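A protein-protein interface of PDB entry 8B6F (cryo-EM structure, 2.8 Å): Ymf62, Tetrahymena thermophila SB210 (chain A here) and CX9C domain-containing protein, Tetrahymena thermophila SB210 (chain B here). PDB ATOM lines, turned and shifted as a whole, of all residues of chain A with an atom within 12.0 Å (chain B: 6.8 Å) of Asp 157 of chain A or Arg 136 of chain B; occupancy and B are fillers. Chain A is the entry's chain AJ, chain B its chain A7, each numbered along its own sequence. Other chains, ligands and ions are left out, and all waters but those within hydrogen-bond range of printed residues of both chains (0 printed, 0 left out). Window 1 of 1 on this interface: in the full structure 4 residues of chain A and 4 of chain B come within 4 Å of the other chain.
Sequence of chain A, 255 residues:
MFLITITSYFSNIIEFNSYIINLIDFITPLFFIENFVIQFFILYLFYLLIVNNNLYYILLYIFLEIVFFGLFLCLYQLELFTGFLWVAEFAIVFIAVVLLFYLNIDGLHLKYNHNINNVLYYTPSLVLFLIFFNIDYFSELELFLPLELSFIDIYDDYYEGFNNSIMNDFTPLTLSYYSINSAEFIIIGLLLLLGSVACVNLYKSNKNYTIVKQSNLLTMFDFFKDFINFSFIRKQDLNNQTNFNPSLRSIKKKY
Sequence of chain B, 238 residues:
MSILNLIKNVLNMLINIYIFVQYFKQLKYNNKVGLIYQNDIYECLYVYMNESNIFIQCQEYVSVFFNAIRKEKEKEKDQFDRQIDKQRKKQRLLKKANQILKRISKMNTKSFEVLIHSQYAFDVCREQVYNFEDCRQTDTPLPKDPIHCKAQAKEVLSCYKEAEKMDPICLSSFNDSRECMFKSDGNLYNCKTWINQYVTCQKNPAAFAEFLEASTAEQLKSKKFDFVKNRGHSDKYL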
ATOM      1  N   PHE A 151      15.381   5.604 -25.692  1.00  0.00           N
ATOM      2  CA  PHE A 151      15.351   6.687 -24.716  1.00  0.00           C
ATOM      3  C   PHE A 151      14.002   7.374 -24.572  1.00  0.00           C
ATOM      4  O   PHE A 151      13.837   8.155 -23.632  1.00  0.00           O
ATOM      5  CB  PHE A 151      16.398   7.748 -25.081  1.00  0.00           C
ATOM      6  CG  PHE A 151      16.205   8.339 -26.446  1.00  0.00           C
ATOM      7  CD1 PHE A 151      16.740   7.719 -27.563  1.00  0.00           C
ATOM      8  CD2 PHE A 151      15.490   9.512 -26.615  1.00  0.00           C
ATOM      9  CE1 PHE A 151      16.564   8.257 -28.822  1.00  0.00           C
ATOM     10  CE2 PHE A 151      15.311  10.055 -27.874  1.00  0.00           C
ATOM     11  CZ  PHE A 151      15.850   9.427 -28.977  1.00  0.00           C
ATOM     12  N   ILE A 152      13.040   7.125 -25.459  1.00  0.00           N
ATOM     13  CA  ILE A 152      11.807   7.906 -25.450  1.00  0.00           C
ATOM     14  C   ILE A 152      10.993   7.630 -24.191  1.00  0.00           C
ATOM     15  O   ILE A 152      10.332   8.527 -23.658  1.00  0.00           O
ATOM     16  CB  ILE A 152      10.996   7.633 -26.730  1.00  0.00           C
ATOM     17  CG1 ILE A 152       9.793   8.576 -26.816  1.00  0.00           C
ATOM     18  CG2 ILE A 152      10.536   6.185 -26.778  1.00  0.00           C
ATOM     19  CD1 ILE A 152      10.154  10.053 -26.809  1.00  0.00           C
ATOM     20  N   ASP A 153      11.017   6.389 -23.701  1.00  0.00           N
ATOM     21  CA  ASP A 153      10.206   6.038 -22.540  1.00  0.00           C
ATOM     22  C   ASP A 153      10.554   6.876 -21.316  1.00  0.00           C
ATOM     23  O   ASP A 153       9.720   7.006 -20.413  1.00  0.00           O
ATOM     24  CB  ASP A 153      10.372   4.553 -22.213  1.00  0.00           C
ATOM     25  CG  ASP A 153       9.819   3.653 -23.299  1.00  0.00           C
ATOM     26  OD1 ASP A 153       8.879   4.077 -24.003  1.00  0.00           O
ATOM     27  OD2 ASP A 153      10.326   2.523 -23.453  1.00  0.00           O
ATOM     28  N   ILE A 154      11.759   7.443 -21.261  1.00  0.00           N
ATOM     29  CA  ILE A 154      12.129   8.294 -20.136  1.00  0.00           C
ATOM     30  C   ILE A 154      11.546   9.696 -20.274  1.00  0.00           C
ATOM     31  O   ILE A 154      11.439  10.415 -19.275  1.00  0.00           O
ATOM     32  CB  ILE A 154      13.662   8.367 -19.990  1.00  0.00           C
ATOM     33  CG1 ILE A 154      14.259   6.990 -19.675  1.00  0.00           C
ATOM     34  CG2 ILE A 154      14.073   9.347 -18.896  1.00  0.00           C
ATOM     35  CD1 ILE A 154      14.420   6.061 -20.870  1.00  0.00           C
ATOM     36  N   TYR A 155      11.151  10.099 -21.479  1.00  0.00           N
ATOM     37  CA  TYR A 155      10.618  11.440 -21.678  1.00  0.00           C
ATOM     38  C   TYR A 155       9.309  11.620 -20.922  1.00  0.00           C
ATOM     39  O   TYR A 155       8.440  10.745 -20.932  1.00  0.00           O
ATOM     40  CB  TYR A 155      10.405  11.705 -23.169  1.00  0.00           C
ATOM     41  CG  TYR A 155       9.800  13.057 -23.466  1.00  0.00           C
ATOM     42  CD1 TYR A 155      10.602  14.180 -23.615  1.00  0.00           C
ATOM     43  CD2 TYR A 155       8.429  13.206 -23.612  1.00  0.00           C
ATOM     44  CE1 TYR A 155      10.053  15.416 -23.888  1.00  0.00           C
ATOM     45  CE2 TYR A 155       7.869  14.437 -23.885  1.00  0.00           C
ATOM     46  CZ  TYR A 155       8.687  15.538 -24.023  1.00  0.00           C
ATOM     47  OH  TYR A 155       8.132  16.767 -24.297  1.00  0.00           O
ATOM     48  N   ASP A 156       9.168  12.772 -20.269  1.00  0.00           N
ATOM     49  CA  ASP A 156       7.968  13.119 -19.522  1.00  0.00           C
ATOM     50  C   ASP A 156       7.514  14.514 -19.917  1.00  0.00           C
ATOM     51  O   ASP A 156       8.334  15.423 -20.077  1.00  0.00           O
ATOM     52  CB  ASP A 156       8.210  13.063 -18.010  1.00  0.00           C
ATOM     53  CG  ASP A 156       8.597  11.678 -17.532  1.00  0.00           C
ATOM     54  OD1 ASP A 156       8.141  10.691 -18.145  1.00  0.00           O
ATOM     55  OD2 ASP A 156       9.353  11.577 -16.544  1.00  0.00           O
ATOM     56  N   ASP A 157       6.205  14.681 -20.067  1.00  0.00           N
ATOM     57  CA  ASP A 157       5.598  15.953 -20.449  1.00  0.00           C
ATOM     58  C   ASP A 157       4.865  16.505 -19.232  1.00  0.00           C
ATOM     59  O   ASP A 157       3.714  16.144 -18.972  1.00  0.00           O
ATOM     60  CB  ASP A 157       4.656  15.766 -21.634  1.00  0.00           C
ATOM     61  CG  ASP A 157       4.155  17.079 -22.192  1.00  0.00           C
ATOM     62  OD1 ASP A 157       4.552  18.140 -21.666  1.00  0.00           O
ATOM     63  OD2 ASP A 157       3.362  17.054 -23.155  1.00  0.00           O
ATOM     64  N   TYR A 158       5.542  17.376 -18.479  1.00  0.00           N
ATOM     65  CA  TYR A 158       4.973  17.867 -17.229  1.00  0.00           C
ATOM     66  C   TYR A 158       3.859  18.875 -17.469  1.00  0.00           C
ATOM     67  O   TYR A 158       2.910  18.941 -16.680  1.00  0.00           O
ATOM     68  CB  TYR A 158       6.071  18.476 -16.359  1.00  0.00           C
ATOM     69  CG  TYR A 158       7.081  17.455 -15.902  1.00  0.00           C
ATOM     70  CD1 TYR A 158       8.182  17.143 -16.683  1.00  0.00           C
ATOM     71  CD2 TYR A 158       6.922  16.790 -14.693  1.00  0.00           C
ATOM     72  CE1 TYR A 158       9.102  16.205 -16.274  1.00  0.00           C
ATOM     73  CE2 TYR A 158       7.837  15.849 -14.273  1.00  0.00           C
ATOM     74  CZ  TYR A 158       8.925  15.561 -15.069  1.00  0.00           C
ATOM     75  OH  TYR A 158       9.839  14.624 -14.656  1.00  0.00           O
ATOM     76  N   TYR A 159       3.948  19.666 -18.539  1.00  0.00           N
ATOM     77  CA  TYR A 159       2.868  20.595 -18.851  1.00  0.00           C
ATOM     78  C   TYR A 159       1.575  19.845 -19.138  1.00  0.00           C
ATOM     79  O   TYR A 159       0.516  20.172 -18.590  1.00  0.00           O
ATOM     80  CB  TYR A 159       3.257  21.488 -20.027  1.00  0.00           C
ATOM     81  CG  TYR A 159       4.095  22.674 -19.615  1.00  0.00           C
ATOM     82  CD1 TYR A 159       5.477  22.580 -19.532  1.00  0.00           C
ATOM     83  CD2 TYR A 159       3.499  23.885 -19.294  1.00  0.00           C
ATOM     84  CE1 TYR A 159       6.241  23.667 -19.149  1.00  0.00           C
ATOM     85  CE2 TYR A 159       4.251  24.974 -18.912  1.00  0.00           C
ATOM     86  CZ  TYR A 159       5.622  24.859 -18.841  1.00  0.00           C
ATOM     87  OH  TYR A 159       6.371  25.945 -18.460  1.00  0.00           O
ATOM     88  N   GLU A 160       1.640  18.837 -20.006  1.00  0.00           N
ATOM     89  CA  GLU A 160       0.472  18.000 -20.250  1.00  0.00           C
ATOM     90  C   GLU A 160       0.060  17.255 -18.990  1.00  0.00           C
ATOM     91  O   GLU A 160      -1.132  17.011 -18.775  1.00  0.00           O
ATOM     92  CB  GLU A 160       0.757  17.018 -21.386  1.00  0.00           C
ATOM     93  CG  GLU A 160      -0.477  16.300 -21.923  1.00  0.00           C
ATOM     94  CD  GLU A 160      -0.912  15.130 -21.060  1.00  0.00           C
ATOM     95  OE1 GLU A 160      -0.113  14.682 -20.212  1.00  0.00           O
ATOM     96  OE2 GLU A 160      -2.052  14.653 -21.235  1.00  0.00           O
ATOM     97  N   GLY A 161       1.026  16.885 -18.149  1.00  0.00           N
ATOM     98  CA  GLY A 161       0.691  16.188 -16.919  1.00  0.00           C
ATOM     99  C   GLY A 161      -0.170  17.019 -15.987  1.00  0.00           C
ATOM    100  O   GLY A 161      -1.174  16.538 -15.458  1.00  0.00           O
ATOM    101  N   PHE A 162       0.206  18.279 -15.775  1.00  0.00           N
ATOM    102  CA  PHE A 162      -0.581  19.135 -14.897  1.00  0.00           C
ATOM    103  C   PHE A 162      -1.850  19.645 -15.563  1.00  0.00           C
ATOM    104  O   PHE A 162      -2.778  20.057 -14.858  1.00  0.00           O
ATOM    105  CB  PHE A 162       0.274  20.307 -14.396  1.00  0.00           C
ATOM    106  CG  PHE A 162       0.114  21.574 -15.187  1.00  0.00           C
ATOM    107  CD1 PHE A 162      -0.924  22.454 -14.928  1.00  0.00           C
ATOM    108  CD2 PHE A 162       1.042  21.912 -16.153  1.00  0.00           C
ATOM    109  CE1 PHE A 162      -1.054  23.624 -15.650  1.00  0.00           C
ATOM    110  CE2 PHE A 162       0.921  23.080 -16.878  1.00  0.00           C
ATOM    111  CZ  PHE A 162      -0.129  23.939 -16.626  1.00  0.00           C
ATOM    112  N   ASN A 163      -1.919  19.624 -16.894  1.00  0.00           N
ATOM    113  CA  ASN A 163      -3.165  19.922 -17.587  1.00  0.00           C
ATOM    114  C   ASN A 163      -4.097  18.722 -17.665  1.00  0.00           C
ATOM    115  O   ASN A 163      -5.262  18.889 -18.039  1.00  0.00           O
ATOM    116  CB  ASN A 163      -2.875  20.422 -19.005  1.00  0.00           C
ATOM    117  CG  ASN A 163      -2.313  21.828 -19.025  1.00  0.00           C
ATOM    118  OD1 ASN A 163      -1.232  22.066 -19.564  1.00  0.00           O
ATOM    119  ND2 ASN A 163      -3.042  22.767 -18.437  1.00  0.00           N
ATOM    120  N   ASN A 164      -3.620  17.528 -17.327  1.00  0.00           N
ATOM    121  CA  ASN A 164      -4.428  16.320 -17.403  1.00  0.00           C
ATOM    122  C   ASN A 164      -5.133  16.090 -16.072  1.00  0.00           C
ATOM    123  O   ASN A 164      -4.491  16.065 -15.018  1.00  0.00           O
ATOM    124  CB  ASN A 164      -3.551  15.118 -17.755  1.00  0.00           C
ATOM    125  CG  ASN A 164      -4.359  13.891 -18.116  1.00  0.00           C
ATOM    126  OD1 ASN A 164      -5.491  13.725 -17.667  1.00  0.00           O
ATOM    127  ND2 ASN A 164      -3.779  13.021 -18.933  1.00  0.00           N
ATOM    128  N   SER A 165      -6.452  15.920 -16.126  1.00  0.00           N
ATOM    129  CA  SER A 165      -7.263  15.692 -14.938  1.00  0.00           C
ATOM    130  C   SER A 165      -7.845  14.288 -14.873  1.00  0.00           C
ATOM    131  O   SER A 165      -8.611  13.993 -13.950  1.00  0.00           O
ATOM    132  CB  SER A 165      -8.395  16.724 -14.872  1.00  0.00           C
ATOM    133  OG  SER A 165      -9.243  16.623 -16.004  1.00  0.00           O
ATOM    134  N   ILE A 166      -7.504  13.414 -15.819  1.00  0.00           N
ATOM    135  CA  ILE A 166      -8.066  12.071 -15.837  1.00  0.00           C
ATOM    136  C   ILE A 166      -7.531  11.266 -14.660  1.00  0.00           C
ATOM    137  O   ILE A 166      -6.383  11.433 -14.228  1.00  0.00           O
ATOM    138  CB  ILE A 166      -7.748  11.382 -17.178  1.00  0.00           C
ATOM    139  CG1 ILE A 166      -8.392  12.156 -18.332  1.00  0.00           C
ATOM    140  CG2 ILE A 166      -8.232   9.937 -17.176  1.00  0.00           C
ATOM    141  CD1 ILE A 166      -7.853  11.781 -19.692  1.00  0.00           C
ATOM    142  N   VAL B 129      11.340  31.686 -17.486  1.00  0.00           N
ATOM    143  CA  VAL B 129      10.216  30.765 -17.618  1.00  0.00           C
ATOM    144  C   VAL B 129       9.319  31.204 -18.767  1.00  0.00           C
ATOM    145  O   VAL B 129       8.858  30.379 -19.564  1.00  0.00           O
ATOM    146  CB  VAL B 129       9.440  30.666 -16.291  1.00  0.00           C
ATOM    147  CG1 VAL B 129       8.166  29.848 -16.468  1.00  0.00           C
ATOM    148  CG2 VAL B 129      10.312  30.051 -15.214  1.00  0.00           C
ATOM    149  N   ASN B 131      10.210  32.947 -21.412  1.00  0.00           N
ATOM    150  CA  ASN B 131      10.901  32.665 -22.663  1.00  0.00           C
ATOM    151  C   ASN B 131      10.788  31.192 -23.028  1.00  0.00           C
ATOM    152  O   ASN B 131      10.520  30.849 -24.185  1.00  0.00           O
ATOM    153  CB  ASN B 131      12.370  33.075 -22.557  1.00  0.00           C
ATOM    154  CG  ASN B 131      12.548  34.574 -22.452  1.00  0.00           C
ATOM    155  OD1 ASN B 131      11.750  35.345 -22.982  1.00  0.00           O
ATOM    156  ND2 ASN B 131      13.602  34.996 -21.764  1.00  0.00           N
ATOM    157  N   PHE B 132      10.996  30.306 -22.053  1.00  0.00           N
ATOM    158  CA  PHE B 132      10.882  28.876 -22.318  1.00  0.00           C
ATOM    159  C   PHE B 132       9.473  28.509 -22.763  1.00  0.00           C
ATOM    160  O   PHE B 132       9.294  27.756 -23.727  1.00  0.00           O
ATOM    161  CB  PHE B 132      11.279  28.087 -21.069  1.00  0.00           C
ATOM    162  CG  PHE B 132      11.096  26.605 -21.203  1.00  0.00           C
ATOM    163  CD1 PHE B 132      11.923  25.863 -22.028  1.00  0.00           C
ATOM    164  CD2 PHE B 132      10.110  25.951 -20.487  1.00  0.00           C
ATOM    165  CE1 PHE B 132      11.761  24.498 -22.144  1.00  0.00           C
ATOM    166  CE2 PHE B 132       9.944  24.588 -20.599  1.00  0.00           C
ATOM    167  CZ  PHE B 132      10.771  23.859 -21.429  1.00  0.00           C
ATOM    168  N   GLU B 133       8.459  29.044 -22.082  1.00  0.00           N
ATOM    169  CA  GLU B 133       7.076  28.739 -22.437  1.00  0.00           C
ATOM    170  C   GLU B 133       6.752  29.217 -23.847  1.00  0.00           C
ATOM    171  O   GLU B 133       6.143  28.488 -24.636  1.00  0.00           O
ATOM    172  CB  GLU B 133       6.123  29.365 -21.422  1.00  0.00           C
ATOM    173  CG  GLU B 133       6.181  28.700 -20.058  1.00  0.00           C
ATOM    174  CD  GLU B 133       5.255  29.351 -19.055  1.00  0.00           C
ATOM    175  OE1 GLU B 133       4.477  30.242 -19.453  1.00  0.00           O
ATOM    176  OE2 GLU B 133       5.304  28.973 -17.865  1.00  0.00           O
ATOM    177  N   ASP B 134       7.159  30.441 -24.185  1.00  0.00           N
ATOM    178  CA  ASP B 134       6.917  30.959 -25.528  1.00  0.00           C
ATOM    179  C   ASP B 134       7.603  30.106 -26.584  1.00  0.00           C
ATOM    180  O   ASP B 134       7.029  29.836 -27.644  1.00  0.00           O
ATOM    181  CB  ASP B 134       7.399  32.406 -25.629  1.00  0.00           C
ATOM    182  CG  ASP B 134       6.477  33.378 -24.932  1.00  0.00           C
ATOM    183  OD1 ASP B 134       6.317  33.269 -23.700  1.00  0.00           O
ATOM    184  OD2 ASP B 134       5.912  34.254 -25.616  1.00  0.00           O
ATOM    185  N   CYS B 135       8.833  29.672 -26.315  1.00  0.00           N
ATOM    186  CA  CYS B 135       9.545  28.834 -27.271  1.00  0.00           C
ATOM    187  C   CYS B 135       8.826  27.508 -27.494  1.00  0.00           C
ATOM    188  O   CYS B 135       8.733  27.028 -28.629  1.00  0.00           O
ATOM    189  CB  CYS B 135      10.978  28.605 -26.792  1.00  0.00           C
ATOM    190  SG  CYS B 135      12.065  27.889 -28.033  1.00  0.00           S
ATOM    191  N   ARG B 136       8.311  26.899 -26.425  1.00  0.00           N
ATOM    192  CA  ARG B 136       7.671  25.593 -26.531  1.00  0.00           C
ATOM    193  C   ARG B 136       6.218  25.662 -26.985  1.00  0.00           C
ATOM    194  O   ARG B 136       5.620  24.611 -27.233  1.00  0.00           O
ATOM    195  CB  ARG B 136       7.738  24.861 -25.187  1.00  0.00           C
ATOM    196  CG  ARG B 136       6.983  25.560 -24.072  1.00  0.00           C
ATOM    197  CD  ARG B 136       7.051  24.796 -22.760  1.00  0.00           C
ATOM    198  NE  ARG B 136       6.154  23.648 -22.758  1.00  0.00           N
ATOM    199  CZ  ARG B 136       6.495  22.419 -23.120  1.00  0.00           C
ATOM    200  NH1 ARG B 136       7.722  22.128 -23.522  1.00  0.00           N
ATOM    201  NH2 ARG B 136       5.579  21.455 -23.082  1.00  0.00           N
ATOM    202  N   GLN B 137       5.634  26.853 -27.095  1.00  0.00           N
ATOM    203  CA  GLN B 137       4.241  26.963 -27.512  1.00  0.00           C
ATOM    204  C   GLN B 137       4.034  26.329 -28.883  1.00  0.00           C
ATOM    205  O   GLN B 137       4.884  26.433 -29.772  1.00  0.00           O
ATOM    206  CB  GLN B 137       3.814  28.431 -27.542  1.00  0.00           C
ATOM    207  CG  GLN B 137       3.373  28.985 -26.194  1.00  0.00           C
ATOM    208  CD  GLN B 137       2.030  28.452 -25.748  1.00  0.00           C
ATOM    209  OE1 GLN B 137       1.490  27.519 -26.340  1.00  0.00           O
ATOM    210  NE2 GLN B 137       1.475  29.050 -24.701  1.00  0.00           N
ATOM    211  N   THR B 138       2.889  25.669 -29.052  1.00  0.00           N
ATOM    212  CA  THR B 138       2.553  24.974 -30.285  1.00  0.00           C
ATOM    213  C   THR B 138       1.054  25.097 -30.523  1.00  0.00           C
ATOM    214  O   THR B 138       0.288  25.434 -29.618  1.00  0.00           O
ATOM    215  CB  THR B 138       2.968  23.493 -30.222  1.00  0.00           C
ATOM    216  OG1 THR B 138       4.309  23.393 -29.734  1.00  0.00           O
ATOM    217  CG2 THR B 138       2.902  22.836 -31.592  1.00  0.00           C
ATOM    218  N   ASP B 139       0.640  24.829 -31.761  1.00  0.00           N
ATOM    219  CA  ASP B 139      -0.763  24.933 -32.140  1.00  0.00           C
ATOM    220  C   ASP B 139      -1.574  23.694 -31.784  1.00  0.00           C
ATOM    221  O   ASP B 139      -2.796  23.707 -31.958  1.00  0.00           O
ATOM    222  CB  ASP B 139      -0.881  25.198 -33.643  1.00  0.00           C
ATOM    223  CG  ASP B 139      -0.461  24.007 -34.478  1.00  0.00           C
ATOM    224  OD1 ASP B 139       0.383  23.217 -34.006  1.00  0.00           O
ATOM    225  OD2 ASP B 139      -0.971  23.860 -35.608  1.00  0.00           O
ATOM    226  N   THR B 140      -0.937  22.633 -31.310  1.00  0.00           N
ATOM    227  CA  THR B 140      -1.597  21.395 -30.931  1.00  0.00           C
ATOM    228  C   THR B 140      -1.078  20.947 -29.576  1.00  0.00           C
ATOM    229  O   THR B 140       0.026  21.323 -29.169  1.00  0.00           O
ATOM    230  CB  THR B 140      -1.349  20.289 -31.968  1.00  0.00           C
ATOM    231  OG1 THR B 140       0.061  20.084 -32.125  1.00  0.00           O
ATOM    232  CG2 THR B 140      -1.952  20.666 -33.306  1.00  0.00           C
ATOM    233  N   PRO B 141      -1.854  20.141 -28.847  1.00  0.00           N
ATOM    234  CA  PRO B 141      -1.378  19.662 -27.539  1.00  0.00           C
ATOM    235  C   PRO B 141      -0.139  18.791 -27.623  1.00  0.00           C
ATOM    236  O   PRO B 141       0.541  18.613 -26.606  1.00  0.00           O
ATOM    237  CB  PRO B 141      -2.580  18.877 -26.992  1.00  0.00           C
ATOM    238  CG  PRO B 141      -3.348  18.494 -28.185  1.00  0.00           C
ATOM    239  CD  PRO B 141      -3.189  19.612 -29.166  1.00  0.00           C
ATOM    240  N   LEU B 142       0.172  18.237 -28.789  1.00  0.00           N
ATOM    241  CA  LEU B 142       1.368  17.422 -28.916  1.00  0.00           C
ATOM    242  C   LEU B 142       2.601  18.265 -28.600  1.00  0.00           C
ATOM    243  O   LEU B 142       2.705  19.408 -29.059  1.00  0.00           O
ATOM    244  CB  LEU B 142       1.478  16.840 -30.325  1.00  0.00           C
ATOM    245  CG  LEU B 142       0.370  15.875 -30.748  1.00  0.00           C
ATOM    246  CD1 LEU B 142       0.565  15.455 -32.190  1.00  0.00           C
ATOM    247  CD2 LEU B 142       0.326  14.653 -29.844  1.00  0.00           C
ATOM    248  N   PRO B 143       3.555  17.737 -27.838  1.00  0.00           N
ATOM    249  CA  PRO B 143       4.705  18.548 -27.431  1.00  0.00           C
ATOM    250  C   PRO B 143       5.595  18.907 -28.609  1.00  0.00           C
ATOM    251  O   PRO B 143       5.627  18.232 -29.639  1.00  0.00           O
ATOM    252  CB  PRO B 143       5.441  17.648 -26.433  1.00  0.00           C
ATOM    253  CG  PRO B 143       5.056  16.273 -26.816  1.00  0.00           C
ATOM    254  CD  PRO B 143       3.646  16.361 -27.320  1.00  0.00           C
ATOM    255  N   LYS B 144       6.318  20.006 -28.439  1.00  0.00           N
ATOM    256  CA  LYS B 144       7.280  20.474 -29.422  1.00  0.00           C
ATOM    257  C   LYS B 144       8.632  19.808 -29.186  1.00  0.00           C
ATOM    258  O   LYS B 144       8.945  19.351 -28.085  1.00  0.00           O
ATOM    259  CB  LYS B 144       7.416  21.994 -29.347  1.00  0.00           C
ATOM    260  CG  LYS B 144       8.160  22.624 -30.510  1.00  0.00           C
ATOM    261  CD  LYS B 144       8.105  24.141 -30.425  1.00  0.00           C
ATOM    262  CE  LYS B 144       8.781  24.788 -31.619  1.00  0.00           C
ATOM    263  NZ  LYS B 144       8.686  26.274 -31.566  1.00  0.00           N
ATOM    264  N   ASP B 145       9.433  19.763 -30.237  1.00  0.00           N
ATOM    265  CA  ASP B 145      10.734  19.116 -30.149  1.00  0.00           C
ATOM    266  C   ASP B 145      11.623  19.885 -29.174  1.00  0.00           C
ATOM    267  O   ASP B 145      11.798  21.098 -29.333  1.00  0.00           O
ATOM    268  CB  ASP B 145      11.384  19.047 -31.527  1.00  0.00           C
ATOM    269  CG  ASP B 145      12.572  18.106 -31.566  1.00  0.00           C
ATOM    270  OD1 ASP B 145      13.305  18.024 -30.560  1.00  0.00           O
ATOM    271  OD2 ASP B 145      12.772  17.447 -32.606  1.00  0.00           O
ATOM    272  N   CYS B 149      13.951  24.259 -28.012  1.00  0.00           N
ATOM    273  CA  CYS B 149      13.867  24.955 -26.736  1.00  0.00           C
ATOM    274  C   CYS B 149      15.061  24.673 -25.834  1.00  0.00           C
ATOM    275  O   CYS B 149      15.056  25.087 -24.671  1.00  0.00           O
ATOM    276  CB  CYS B 149      12.575  24.567 -26.015  1.00  0.00           C
ATOM    277  SG  CYS B 149      11.146  24.384 -27.105  1.00  0.00           S
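OD1 of Asp 157 of chain A is in salt-bridge range of NH2 of Arg 136 of chain B, 3.7 Å away.
The side-chain carboxylate of Glu 133 of chain B lies close to the side-chain hydroxyl of Tyr 159 of chain A (3.3 Å).
The side-chain hydroxyl (OG1) of Thr 138 of chain B lies within hydrogen-bond range of the backbone carbonyl oxygen (O) of Arg 136 of chain B (3.1 Å).
The side-chain carboxylate (OD1) of Asp 157 of chain A is in hydrogen-bond range of the backbone NH (N) of Glu 160 of chain A.
The backbone carbonyl oxygen (O) of Tyr 159 of chain A sits close to the side-chain amide oxygen (OD1) of Asn 163 of chain A (2.8 Å).
Pro 143 of chain B touches Tyr 155 of chain A (CB to OH, 3.5 Å).
Asp 157 of chain A touches Pro 143 of chain B (OD2 to CB, 3.9 Å).
CD1 of Tyr 159 of chain A touches NE of Arg 136 of chain B (3.5 Å).
Ile 152 of chain A touches none of the printed residues of chain B.
Of the printed residues of chain B, Tyr 155 of chain A touches Pro 143.
Of chain B, only Arg 136 and Pro 143 come within 4 Å of Asp 157 of chain A.
Printed residues of chain B within 4 Å of Tyr 159 of chain A: Glu 133 (3.2 Å) and Arg 136 (3.5 Å).
Asn 131 of chain B touches none of the printed residues of chain A.
Of chain A, only Tyr 159 comes within 4 Å of Glu 133 of chain B.
No residue of chain A comes within 4 Å of Asp 134 of chain B.
Cys 135 of chain B touches none of the printed residues of chain A.
Of the printed residues of chain A, Arg 136 of chain B touches Asp 157 and Tyr 159.
No residue of chain A comes within 4 Å of Gln 137 of chain B.
No residue of chain A comes within 4 Å of Thr 138 of chain B.
No residue of chain A comes within 4 Å of Lys 144 of chain B.
No residue of chain A comes within 4 Å of Cys 149 of chain B.
Of the 17 printed residues of chain B, 3 touch a printed residue of chain A.
Of the 16 printed residues of chain A, 3 touch a printed residue of chain B.
Among the printed residues, 5 pairs touch across the chains.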
